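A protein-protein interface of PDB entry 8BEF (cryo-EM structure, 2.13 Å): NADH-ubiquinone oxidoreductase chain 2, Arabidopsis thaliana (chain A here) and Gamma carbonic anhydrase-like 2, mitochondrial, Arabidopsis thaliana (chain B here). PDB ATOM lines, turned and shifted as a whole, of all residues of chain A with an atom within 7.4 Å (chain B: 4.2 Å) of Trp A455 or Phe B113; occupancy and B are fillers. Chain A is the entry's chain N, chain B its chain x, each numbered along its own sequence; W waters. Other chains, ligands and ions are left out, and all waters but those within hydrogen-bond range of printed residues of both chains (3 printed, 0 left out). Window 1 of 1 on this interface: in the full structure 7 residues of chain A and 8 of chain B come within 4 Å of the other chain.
Phe B113 touches Lys A382.
NZ of Lys A382 touches OH of Tyr B142, 3.8 Å away.
CA of Thr A383 touches CE1 of Phe B113, at 3.9 Å.
Phe B113 touches Trp A455.
Trp A455 touches Tyr B142.
Trp B91 touches Leu A457.
Asp A376 touches none of the printed residues of chain B.
Of the printed residues of chain B, Pro A452 touches Arg B141 (3.4 Å).
Of chain B, only Phe B113 (3.6 Å), Arg B141 (3.3 Å) and Tyr B142 (3.7 Å) come within 4 Å of Trp A455.
Of the printed residues of chain A, Trp B91 touches Leu A457 (3.5 Å).
Phe B113 touches just these residues of chain A: Lys A382, Thr A383 and Trp A455.
The nearest printed residue of chain B that does not touch Trp A455 is Cys B114 (7.0 Å).
The nearest printed residue of chain A that does not touch Trp B91 is Tyr A458 (5.2 Å).
Water W1 bridges the side-chain carboxylate (OD2) of Asp B92 and the backbone carbonyl oxygen (O) of Tyr A458.
Water W2 lies within hydrogen-bond range of OH of Tyr B142 (2.7 Å) and NZ of Lys A382 (3.4 Å).
Water W3 bridges the side-chain hydroxyl of Tyr B142 (3.0 Å) and the side-chain amino group of Lys A382 (3.4 Å).
The backbone carbonyl oxygen of Phe B113 is in hydrogen-bond range of the backbone NH of Tyr B142 (3.0 Å).
NE1 of Trp A455 is in hydrogen-bond range of O of Pro A452, at 3.1 Å.
OG of Ser B115 is in hydrogen-bond range of N of Tyr B142 (3.3 Å).
Hydrophobic or aromatic side chains of chain A within 4 Å of the printed part of chain B: Trp A455 and Leu A457.
Of the 8 printed residues of chain B, 4 touch a printed residue of chain A.
Printed residues of chain B that touch a printed residue of chain A: Trp B91, Phe B113, Arg B141 and Tyr B142.
Hydrophobic or aromatic side chains of chain B that line the printed part of chain A: Trp B91, Phe B113 and Tyr B142.
Among the printed residues, 9 pairs touch across the chains.
NH2 of Arg B141 sits close to NE1 of Trp A455.
The guanidinium group of Arg B141 sits at hydrogen-bond distance from the backbone carbonyl oxygen of Pro A452 (3.4 Å).
O of Arg A453 is in hydrogen-bond range of NH2 of Arg B141 (3.0 Å).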
ATOM      1  N   ASP A 376     -13.888  -3.196   9.321  1.00  0.00           N
ATOM      2  CA  ASP A 376     -13.546  -3.790  10.611  1.00  0.00           C
ATOM      3  C   ASP A 376     -12.047  -3.748  10.889  1.00  0.00           C
ATOM      4  O   ASP A 376     -11.637  -3.937  12.037  1.00  0.00           O
ATOM      5  CB  ASP A 376     -14.036  -5.240  10.683  1.00  0.00           C
ATOM      6  CG  ASP A 376     -15.551  -5.355  10.713  1.00  0.00           C
ATOM      7  OD1 ASP A 376     -16.222  -4.382  11.123  1.00  0.00           O
ATOM      8  OD2 ASP A 376     -16.072  -6.424  10.327  1.00  0.00           O
ATOM      9  N   GLY A 378     -10.234  -1.146  10.840  1.00  0.00           N
ATOM     10  CA  GLY A 378      -9.832   0.195  11.230  1.00  0.00           C
ATOM     11  C   GLY A 378      -8.961   0.182  12.474  1.00  0.00           C
ATOM     12  O   GLY A 378      -9.158  -0.619  13.388  1.00  0.00           O
ATOM     13  N   ALA A 379      -7.970   1.076  12.490  1.00  0.00           N
ATOM     14  CA  ALA A 379      -7.043   1.261  13.607  1.00  0.00           C
ATOM     15  C   ALA A 379      -6.184   0.025  13.884  1.00  0.00           C
ATOM     16  O   ALA A 379      -5.584  -0.080  14.957  1.00  0.00           O
ATOM     17  CB  ALA A 379      -7.786   1.681  14.883  1.00  0.00           C
ATOM     18  N   LEU A 380      -6.101  -0.913  12.935  1.00  0.00           N
ATOM     19  CA  LEU A 380      -5.271  -2.098  13.141  1.00  0.00           C
ATOM     20  C   LEU A 380      -3.796  -1.744  13.281  1.00  0.00           C
ATOM     21  O   LEU A 380      -3.065  -2.427  14.004  1.00  0.00           O
ATOM     22  CB  LEU A 380      -5.465  -3.096  12.000  1.00  0.00           C
ATOM     23  CG  LEU A 380      -4.891  -4.494  12.241  1.00  0.00           C
ATOM     24  CD1 LEU A 380      -5.353  -5.058  13.583  1.00  0.00           C
ATOM     25  CD2 LEU A 380      -5.247  -5.438  11.101  1.00  0.00           C
ATOM     26  N   ALA A 381      -3.341  -0.683  12.611  1.00  0.00           N
ATOM     27  CA  ALA A 381      -1.958  -0.246  12.781  1.00  0.00           C
ATOM     28  C   ALA A 381      -1.678   0.243  14.196  1.00  0.00           C
ATOM     29  O   ALA A 381      -0.509   0.374  14.574  1.00  0.00           O
ATOM     30  CB  ALA A 381      -1.616   0.851  11.775  1.00  0.00           C
ATOM     31  N   LYS A 382      -2.718   0.517  14.982  1.00  0.00           N
ATOM     32  CA  LYS A 382      -2.537   0.910  16.373  1.00  0.00           C
ATOM     33  C   LYS A 382      -2.644  -0.283  17.317  1.00  0.00           C
ATOM     34  O   LYS A 382      -1.829  -0.428  18.232  1.00  0.00           O
ATOM     35  CB  LYS A 382      -3.563   1.986  16.749  1.00  0.00           C
ATOM     36  CG  LYS A 382      -3.555   3.205  15.831  1.00  0.00           C
ATOM     37  CD  LYS A 382      -2.913   4.429  16.467  1.00  0.00           C
ATOM     38  CE  LYS A 382      -1.597   4.121  17.158  1.00  0.00           C
ATOM     39  NZ  LYS A 382      -1.028   5.321  17.834  1.00  0.00           N
ATOM     40  N   THR A 383      -3.642  -1.146  17.109  1.00  0.00           N
ATOM     41  CA  THR A 383      -3.877  -2.264  18.015  1.00  0.00           C
ATOM     42  C   THR A 383      -2.956  -3.452  17.761  1.00  0.00           C
ATOM     43  O   THR A 383      -2.778  -4.276  18.662  1.00  0.00           O
ATOM     44  CB  THR A 383      -5.343  -2.709  17.937  1.00  0.00           C
ATOM     45  OG1 THR A 383      -5.635  -3.212  16.627  1.00  0.00           O
ATOM     46  CG2 THR A 383      -6.265  -1.542  18.245  1.00  0.00           C
ATOM     47  N   ASN A 384      -2.366  -3.560  16.571  1.00  0.00           N
ATOM     48  CA  ASN A 384      -1.382  -4.601  16.289  1.00  0.00           C
ATOM     49  C   ASN A 384      -0.494  -4.140  15.137  1.00  0.00           C
ATOM     50  O   ASN A 384      -0.734  -4.501  13.978  1.00  0.00           O
ATOM     51  CB  ASN A 384      -2.072  -5.933  15.973  1.00  0.00           C
ATOM     52  CG  ASN A 384      -1.120  -7.121  16.030  1.00  0.00           C
ATOM     53  OD1 ASN A 384       0.096  -6.966  15.951  1.00  0.00           O
ATOM     54  ND2 ASN A 384      -1.679  -8.316  16.183  1.00  0.00           N
ATOM     55  N   PRO A 385       0.530  -3.329  15.425  1.00  0.00           N
ATOM     56  CA  PRO A 385       1.319  -2.722  14.333  1.00  0.00           C
ATOM     57  C   PRO A 385       1.972  -3.726  13.394  1.00  0.00           C
ATOM     58  O   PRO A 385       1.906  -3.552  12.171  1.00  0.00           O
ATOM     59  CB  PRO A 385       2.360  -1.883  15.092  1.00  0.00           C
ATOM     60  CG  PRO A 385       1.736  -1.613  16.424  1.00  0.00           C
ATOM     61  CD  PRO A 385       0.934  -2.833  16.752  1.00  0.00           C
ATOM     62  N   ASP A 450      -7.227   5.741   8.706  1.00  0.00           N
ATOM     63  CA  ASP A 450      -8.541   6.063   9.238  1.00  0.00           C
ATOM     64  C   ASP A 450      -8.501   6.208  10.755  1.00  0.00           C
ATOM     65  O   ASP A 450      -7.677   5.598  11.439  1.00  0.00           O
ATOM     66  CB  ASP A 450      -9.556   4.988   8.842  1.00  0.00           C
ATOM     67  CG  ASP A 450     -10.101   5.188   7.440  1.00  0.00           C
ATOM     68  OD1 ASP A 450     -10.394   4.183   6.763  1.00  0.00           O
ATOM     69  OD2 ASP A 450     -10.238   6.352   7.011  1.00  0.00           O
ATOM     70  N   THR A 451      -9.412   7.029  11.276  1.00  0.00           N
ATOM     71  CA  THR A 451      -9.573   7.238  12.715  1.00  0.00           C
ATOM     72  C   THR A 451     -11.034   6.994  13.075  1.00  0.00           C
ATOM     73  O   THR A 451     -11.812   7.939  13.247  1.00  0.00           O
ATOM     74  CB  THR A 451      -9.123   8.641  13.128  1.00  0.00           C
ATOM     75  OG1 THR A 451      -9.743   9.615  12.279  1.00  0.00           O
ATOM     76  CG2 THR A 451      -7.614   8.771  13.009  1.00  0.00           C
ATOM     77  N   PRO A 452     -11.442   5.732  13.192  1.00  0.00           N
ATOM     78  CA  PRO A 452     -12.845   5.436  13.500  1.00  0.00           C
ATOM     79  C   PRO A 452     -13.178   5.726  14.956  1.00  0.00           C
ATOM     80  O   PRO A 452     -12.313   5.765  15.831  1.00  0.00           O
ATOM     81  CB  PRO A 452     -12.981   3.940  13.195  1.00  0.00           C
ATOM     82  CG  PRO A 452     -11.595   3.420  12.982  1.00  0.00           C
ATOM     83  CD  PRO A 452     -10.604   4.524  13.156  1.00  0.00           C
ATOM     84  N   ARG A 453     -14.473   5.929  15.203  1.00  0.00           N
ATOM     85  CA  ARG A 453     -14.933   6.193  16.561  1.00  0.00           C
ATOM     86  C   ARG A 453     -14.924   4.923  17.406  1.00  0.00           C
ATOM     87  O   ARG A 453     -14.548   4.955  18.582  1.00  0.00           O
ATOM     88  CB  ARG A 453     -16.330   6.816  16.524  1.00  0.00           C
ATOM     89  CG  ARG A 453     -17.038   6.881  17.867  1.00  0.00           C
ATOM     90  CD  ARG A 453     -16.239   7.676  18.892  1.00  0.00           C
ATOM     91  NE  ARG A 453     -16.890   7.687  20.198  1.00  0.00           N
ATOM     92  CZ  ARG A 453     -16.717   6.762  21.133  1.00  0.00           C
ATOM     93  NH1 ARG A 453     -15.924   5.723  20.937  1.00  0.00           N
ATOM     94  NH2 ARG A 453     -17.363   6.880  22.290  1.00  0.00           N
ATOM     95  N   THR A 454     -15.328   3.797  16.824  1.00  0.00           N
ATOM     96  CA  THR A 454     -15.328   2.511  17.508  1.00  0.00           C
ATOM     97  C   THR A 454     -14.263   1.614  16.891  1.00  0.00           C
ATOM     98  O   THR A 454     -14.215   1.451  15.668  1.00  0.00           O
ATOM     99  CB  THR A 454     -16.704   1.841  17.428  1.00  0.00           C
ATOM    100  OG1 THR A 454     -17.644   2.579  18.218  1.00  0.00           O
ATOM    101  CG2 THR A 454     -16.643   0.410  17.945  1.00  0.00           C
ATOM    102  N   TRP A 455     -13.409   1.049  17.736  1.00  0.00           N
ATOM    103  CA  TRP A 455     -12.370   0.123  17.311  1.00  0.00           C
ATOM    104  C   TRP A 455     -12.788  -1.308  17.623  1.00  0.00           C
ATOM    105  O   TRP A 455     -13.566  -1.560  18.545  1.00  0.00           O
ATOM    106  CB  TRP A 455     -11.040   0.420  18.009  1.00  0.00           C
ATOM    107  CG  TRP A 455     -10.440   1.766  17.722  1.00  0.00           C
ATOM    108  CD1 TRP A 455     -11.021   2.807  17.064  1.00  0.00           C
ATOM    109  CD2 TRP A 455      -9.135   2.213  18.106  1.00  0.00           C
ATOM    110  NE1 TRP A 455     -10.158   3.873  17.009  1.00  0.00           N
ATOM    111  CE2 TRP A 455      -8.992   3.534  17.642  1.00  0.00           C
ATOM    112  CE3 TRP A 455      -8.070   1.621  18.793  1.00  0.00           C
ATOM    113  CZ2 TRP A 455      -7.828   4.272  17.841  1.00  0.00           C
ATOM    114  CZ3 TRP A 455      -6.916   2.356  18.989  1.00  0.00           C
ATOM    115  CH2 TRP A 455      -6.805   3.668  18.515  1.00  0.00           C
ATOM    116  N   ILE A 456     -12.261  -2.246  16.844  1.00  0.00           N
ATOM    117  CA  ILE A 456     -12.385  -3.668  17.140  1.00  0.00           C
ATOM    118  C   ILE A 456     -11.009  -4.170  17.550  1.00  0.00           C
ATOM    119  O   ILE A 456     -10.041  -4.041  16.791  1.00  0.00           O
ATOM    120  CB  ILE A 456     -12.933  -4.461  15.945  1.00  0.00           C
ATOM    121  CG1 ILE A 456     -14.430  -4.200  15.776  1.00  0.00           C
ATOM    122  CG2 ILE A 456     -12.688  -5.952  16.144  1.00  0.00           C
ATOM    123  CD1 ILE A 456     -14.914  -4.366  14.362  1.00  0.00           C
ATOM    124  N   LEU A 457     -10.918  -4.732  18.750  1.00  0.00           N
ATOM    125  CA  LEU A 457      -9.670  -5.287  19.256  1.00  0.00           C
ATOM    126  C   LEU A 457      -9.642  -6.780  18.954  1.00  0.00           C
ATOM    127  O   LEU A 457     -10.554  -7.512  19.345  1.00  0.00           O
ATOM    128  CB  LEU A 457      -9.538  -5.027  20.757  1.00  0.00           C
ATOM    129  CG  LEU A 457      -9.831  -3.588  21.195  1.00  0.00           C
ATOM    130  CD1 LEU A 457      -9.609  -3.398  22.692  1.00  0.00           C
ATOM    131  CD2 LEU A 457      -8.994  -2.605  20.397  1.00  0.00           C
ATOM    132  N   TYR A 458      -8.596  -7.230  18.268  1.00  0.00           N
ATOM    133  CA  TYR A 458      -8.510  -8.604  17.794  1.00  0.00           C
ATOM    134  C   TYR A 458      -7.653  -9.454  18.724  1.00  0.00           C
ATOM    135  O   TYR A 458      -6.650  -8.985  19.269  1.00  0.00           O
ATOM    136  CB  TYR A 458      -7.950  -8.647  16.370  1.00  0.00           C
ATOM    137  CG  TYR A 458      -8.902  -8.074  15.350  1.00  0.00           C
ATOM    138  CD1 TYR A 458      -9.870  -8.869  14.754  1.00  0.00           C
ATOM    139  CD2 TYR A 458      -8.847  -6.732  14.997  1.00  0.00           C
ATOM    140  CE1 TYR A 458     -10.750  -8.351  13.830  1.00  0.00           C
ATOM    141  CE2 TYR A 458      -9.722  -6.203  14.073  1.00  0.00           C
ATOM    142  CZ  TYR A 458     -10.672  -7.017  13.490  1.00  0.00           C
ATOM    143  OH  TYR A 458     -11.548  -6.494  12.571  1.00  0.00           O
ATOM    144  N   TRP B  91      -7.721  -5.119  28.375  1.00  0.00           N
ATOM    145  CA  TRP B  91      -7.399  -5.211  26.958  1.00  0.00           C
ATOM    146  C   TRP B  91      -5.930  -4.868  26.693  1.00  0.00           C
ATOM    147  O   TRP B  91      -5.169  -4.523  27.597  1.00  0.00           O
ATOM    148  CB  TRP B  91      -8.331  -4.310  26.150  1.00  0.00           C
ATOM    149  CG  TRP B  91      -9.683  -4.908  25.928  1.00  0.00           C
ATOM    150  CD1 TRP B  91     -10.838  -4.578  26.571  1.00  0.00           C
ATOM    151  CD2 TRP B  91     -10.022  -5.949  25.003  1.00  0.00           C
ATOM    152  NE1 TRP B  91     -11.876  -5.344  26.103  1.00  0.00           N
ATOM    153  CE2 TRP B  91     -11.401  -6.195  25.140  1.00  0.00           C
ATOM    154  CE3 TRP B  91      -9.292  -6.697  24.072  1.00  0.00           C
ATOM    155  CZ2 TRP B  91     -12.067  -7.155  24.381  1.00  0.00           C
ATOM    156  CZ3 TRP B  91      -9.954  -7.648  23.319  1.00  0.00           C
ATOM    157  CH2 TRP B  91     -11.329  -7.867  23.479  1.00  0.00           C
ATOM    158  N   ASP B  92      -5.537  -4.961  25.422  1.00  0.00           N
ATOM    159  CA  ASP B  92      -4.142  -4.785  25.033  1.00  0.00           C
ATOM    160  C   ASP B  92      -3.627  -3.398  25.396  1.00  0.00           C
ATOM    161  O   ASP B  92      -4.301  -2.388  25.181  1.00  0.00           O
ATOM    162  CB  ASP B  92      -3.977  -5.016  23.529  1.00  0.00           C
ATOM    163  CG  ASP B  92      -4.135  -6.471  23.139  1.00  0.00           C
ATOM    164  OD1 ASP B  92      -4.091  -7.343  24.032  1.00  0.00           O
ATOM    165  OD2 ASP B  92      -4.296  -6.740  21.932  1.00  0.00           O
ATOM    166  N   GLY B 112     -10.134  -0.462  28.603  1.00  0.00           N
ATOM    167  CA  GLY B 112      -9.936  -0.418  27.170  1.00  0.00           C
ATOM    168  C   GLY B 112      -8.484  -0.326  26.732  1.00  0.00           C
ATOM    169  O   GLY B 112      -7.548  -0.323  27.530  1.00  0.00           O
ATOM    170  N   PHE B 113      -8.315  -0.251  25.414  1.00  0.00           N
ATOM    171  CA  PHE B 113      -6.995  -0.237  24.796  1.00  0.00           C
ATOM    172  C   PHE B 113      -6.154   0.915  25.330  1.00  0.00           C
ATOM    173  O   PHE B 113      -6.576   2.073  25.286  1.00  0.00           O
ATOM    174  CB  PHE B 113      -7.138  -0.128  23.279  1.00  0.00           C
ATOM    175  CG  PHE B 113      -5.830   0.009  22.553  1.00  0.00           C
ATOM    176  CD1 PHE B 113      -5.019  -1.091  22.341  1.00  0.00           C
ATOM    177  CD2 PHE B 113      -5.408   1.245  22.092  1.00  0.00           C
ATOM    178  CE1 PHE B 113      -3.814  -0.964  21.672  1.00  0.00           C
ATOM    179  CE2 PHE B 113      -4.206   1.378  21.425  1.00  0.00           C
ATOM    180  CZ  PHE B 113      -3.408   0.272  21.216  1.00  0.00           C
ATOM    181  N   CYS B 114      -4.965   0.586  25.835  1.00  0.00           N
ATOM    182  CA  CYS B 114      -3.982   1.575  26.283  1.00  0.00           C
ATOM    183  C   CYS B 114      -4.527   2.475  27.392  1.00  0.00           C
ATOM    184  O   CYS B 114      -4.160   3.645  27.487  1.00  0.00           O
ATOM    185  CB  CYS B 114      -3.481   2.421  25.108  1.00  0.00           C
ATOM    186  SG  CYS B 114      -1.764   2.951  25.252  1.00  0.00           S
ATOM    187  N   SER B 115      -5.408   1.945  28.234  1.00  0.00           N
ATOM    188  CA  SER B 115      -5.930   2.679  29.377  1.00  0.00           C
ATOM    189  C   SER B 115      -5.255   2.205  30.659  1.00  0.00           C
ATOM    190  O   SER B 115      -4.677   1.123  30.717  1.00  0.00           O
ATOM    191  CB  SER B 115      -7.450   2.513  29.485  1.00  0.00           C
ATOM    192  OG  SER B 115      -8.105   3.207  28.440  1.00  0.00           O
ATOM    193  N   ARG B 141     -10.804   3.513  25.497  1.00  0.00           N
ATOM    194  CA  ARG B 141      -9.393   3.576  25.151  1.00  0.00           C
ATOM    195  C   ARG B 141      -8.781   4.928  25.514  1.00  0.00           C
ATOM    196  O   ARG B 141      -9.466   5.950  25.581  1.00  0.00           O
ATOM    197  CB  ARG B 141      -9.203   3.307  23.657  1.00  0.00           C
ATOM    198  CG  ARG B 141      -9.857   4.337  22.745  1.00  0.00           C
ATOM    199  CD  ARG B 141      -9.495   4.097  21.287  1.00  0.00           C
ATOM    200  NE  ARG B 141     -10.091   5.087  20.399  1.00  0.00           N
ATOM    201  CZ  ARG B 141     -11.332   5.027  19.935  1.00  0.00           C
ATOM    202  NH1 ARG B 141     -12.143   4.032  20.253  1.00  0.00           N
ATOM    203  NH2 ARG B 141     -11.768   5.990  19.129  1.00  0.00           N
ATOM    204  N   TYR B 142      -7.465   4.913  25.739  1.00  0.00           N
ATOM    205  CA  TYR B 142      -6.689   6.119  26.036  1.00  0.00           C
ATOM    206  C   TYR B 142      -7.262   6.883  27.230  1.00  0.00           C
ATOM    207  O   TYR B 142      -7.340   8.111  27.227  1.00  0.00           O
ATOM    208  CB  TYR B 142      -6.596   7.033  24.809  1.00  0.00           C
ATOM    209  CG  TYR B 142      -5.836   6.447  23.637  1.00  0.00           C
ATOM    210  CD1 TYR B 142      -4.543   5.968  23.793  1.00  0.00           C
ATOM    211  CD2 TYR B 142      -6.411   6.383  22.373  1.00  0.00           C
ATOM    212  CE1 TYR B 142      -3.842   5.434  22.728  1.00  0.00           C
ATOM    213  CE2 TYR B 142      -5.718   5.853  21.298  1.00  0.00           C
ATOM    214  CZ  TYR B 142      -4.433   5.380  21.483  1.00  0.00           C
ATOM    215  OH  TYR B 142      -3.737   4.848  20.421  1.00  0.00           O
HETATM  216  O   HOH W   1      -6.011  -6.097  20.114  1.00  0.00           O
HETATM  217  O   HOH W   2      -4.106   6.594  18.423  1.00  0.00           O
HETATM  218  O   HOH W   3      -1.097   3.538  20.678  1.00  0.00           O
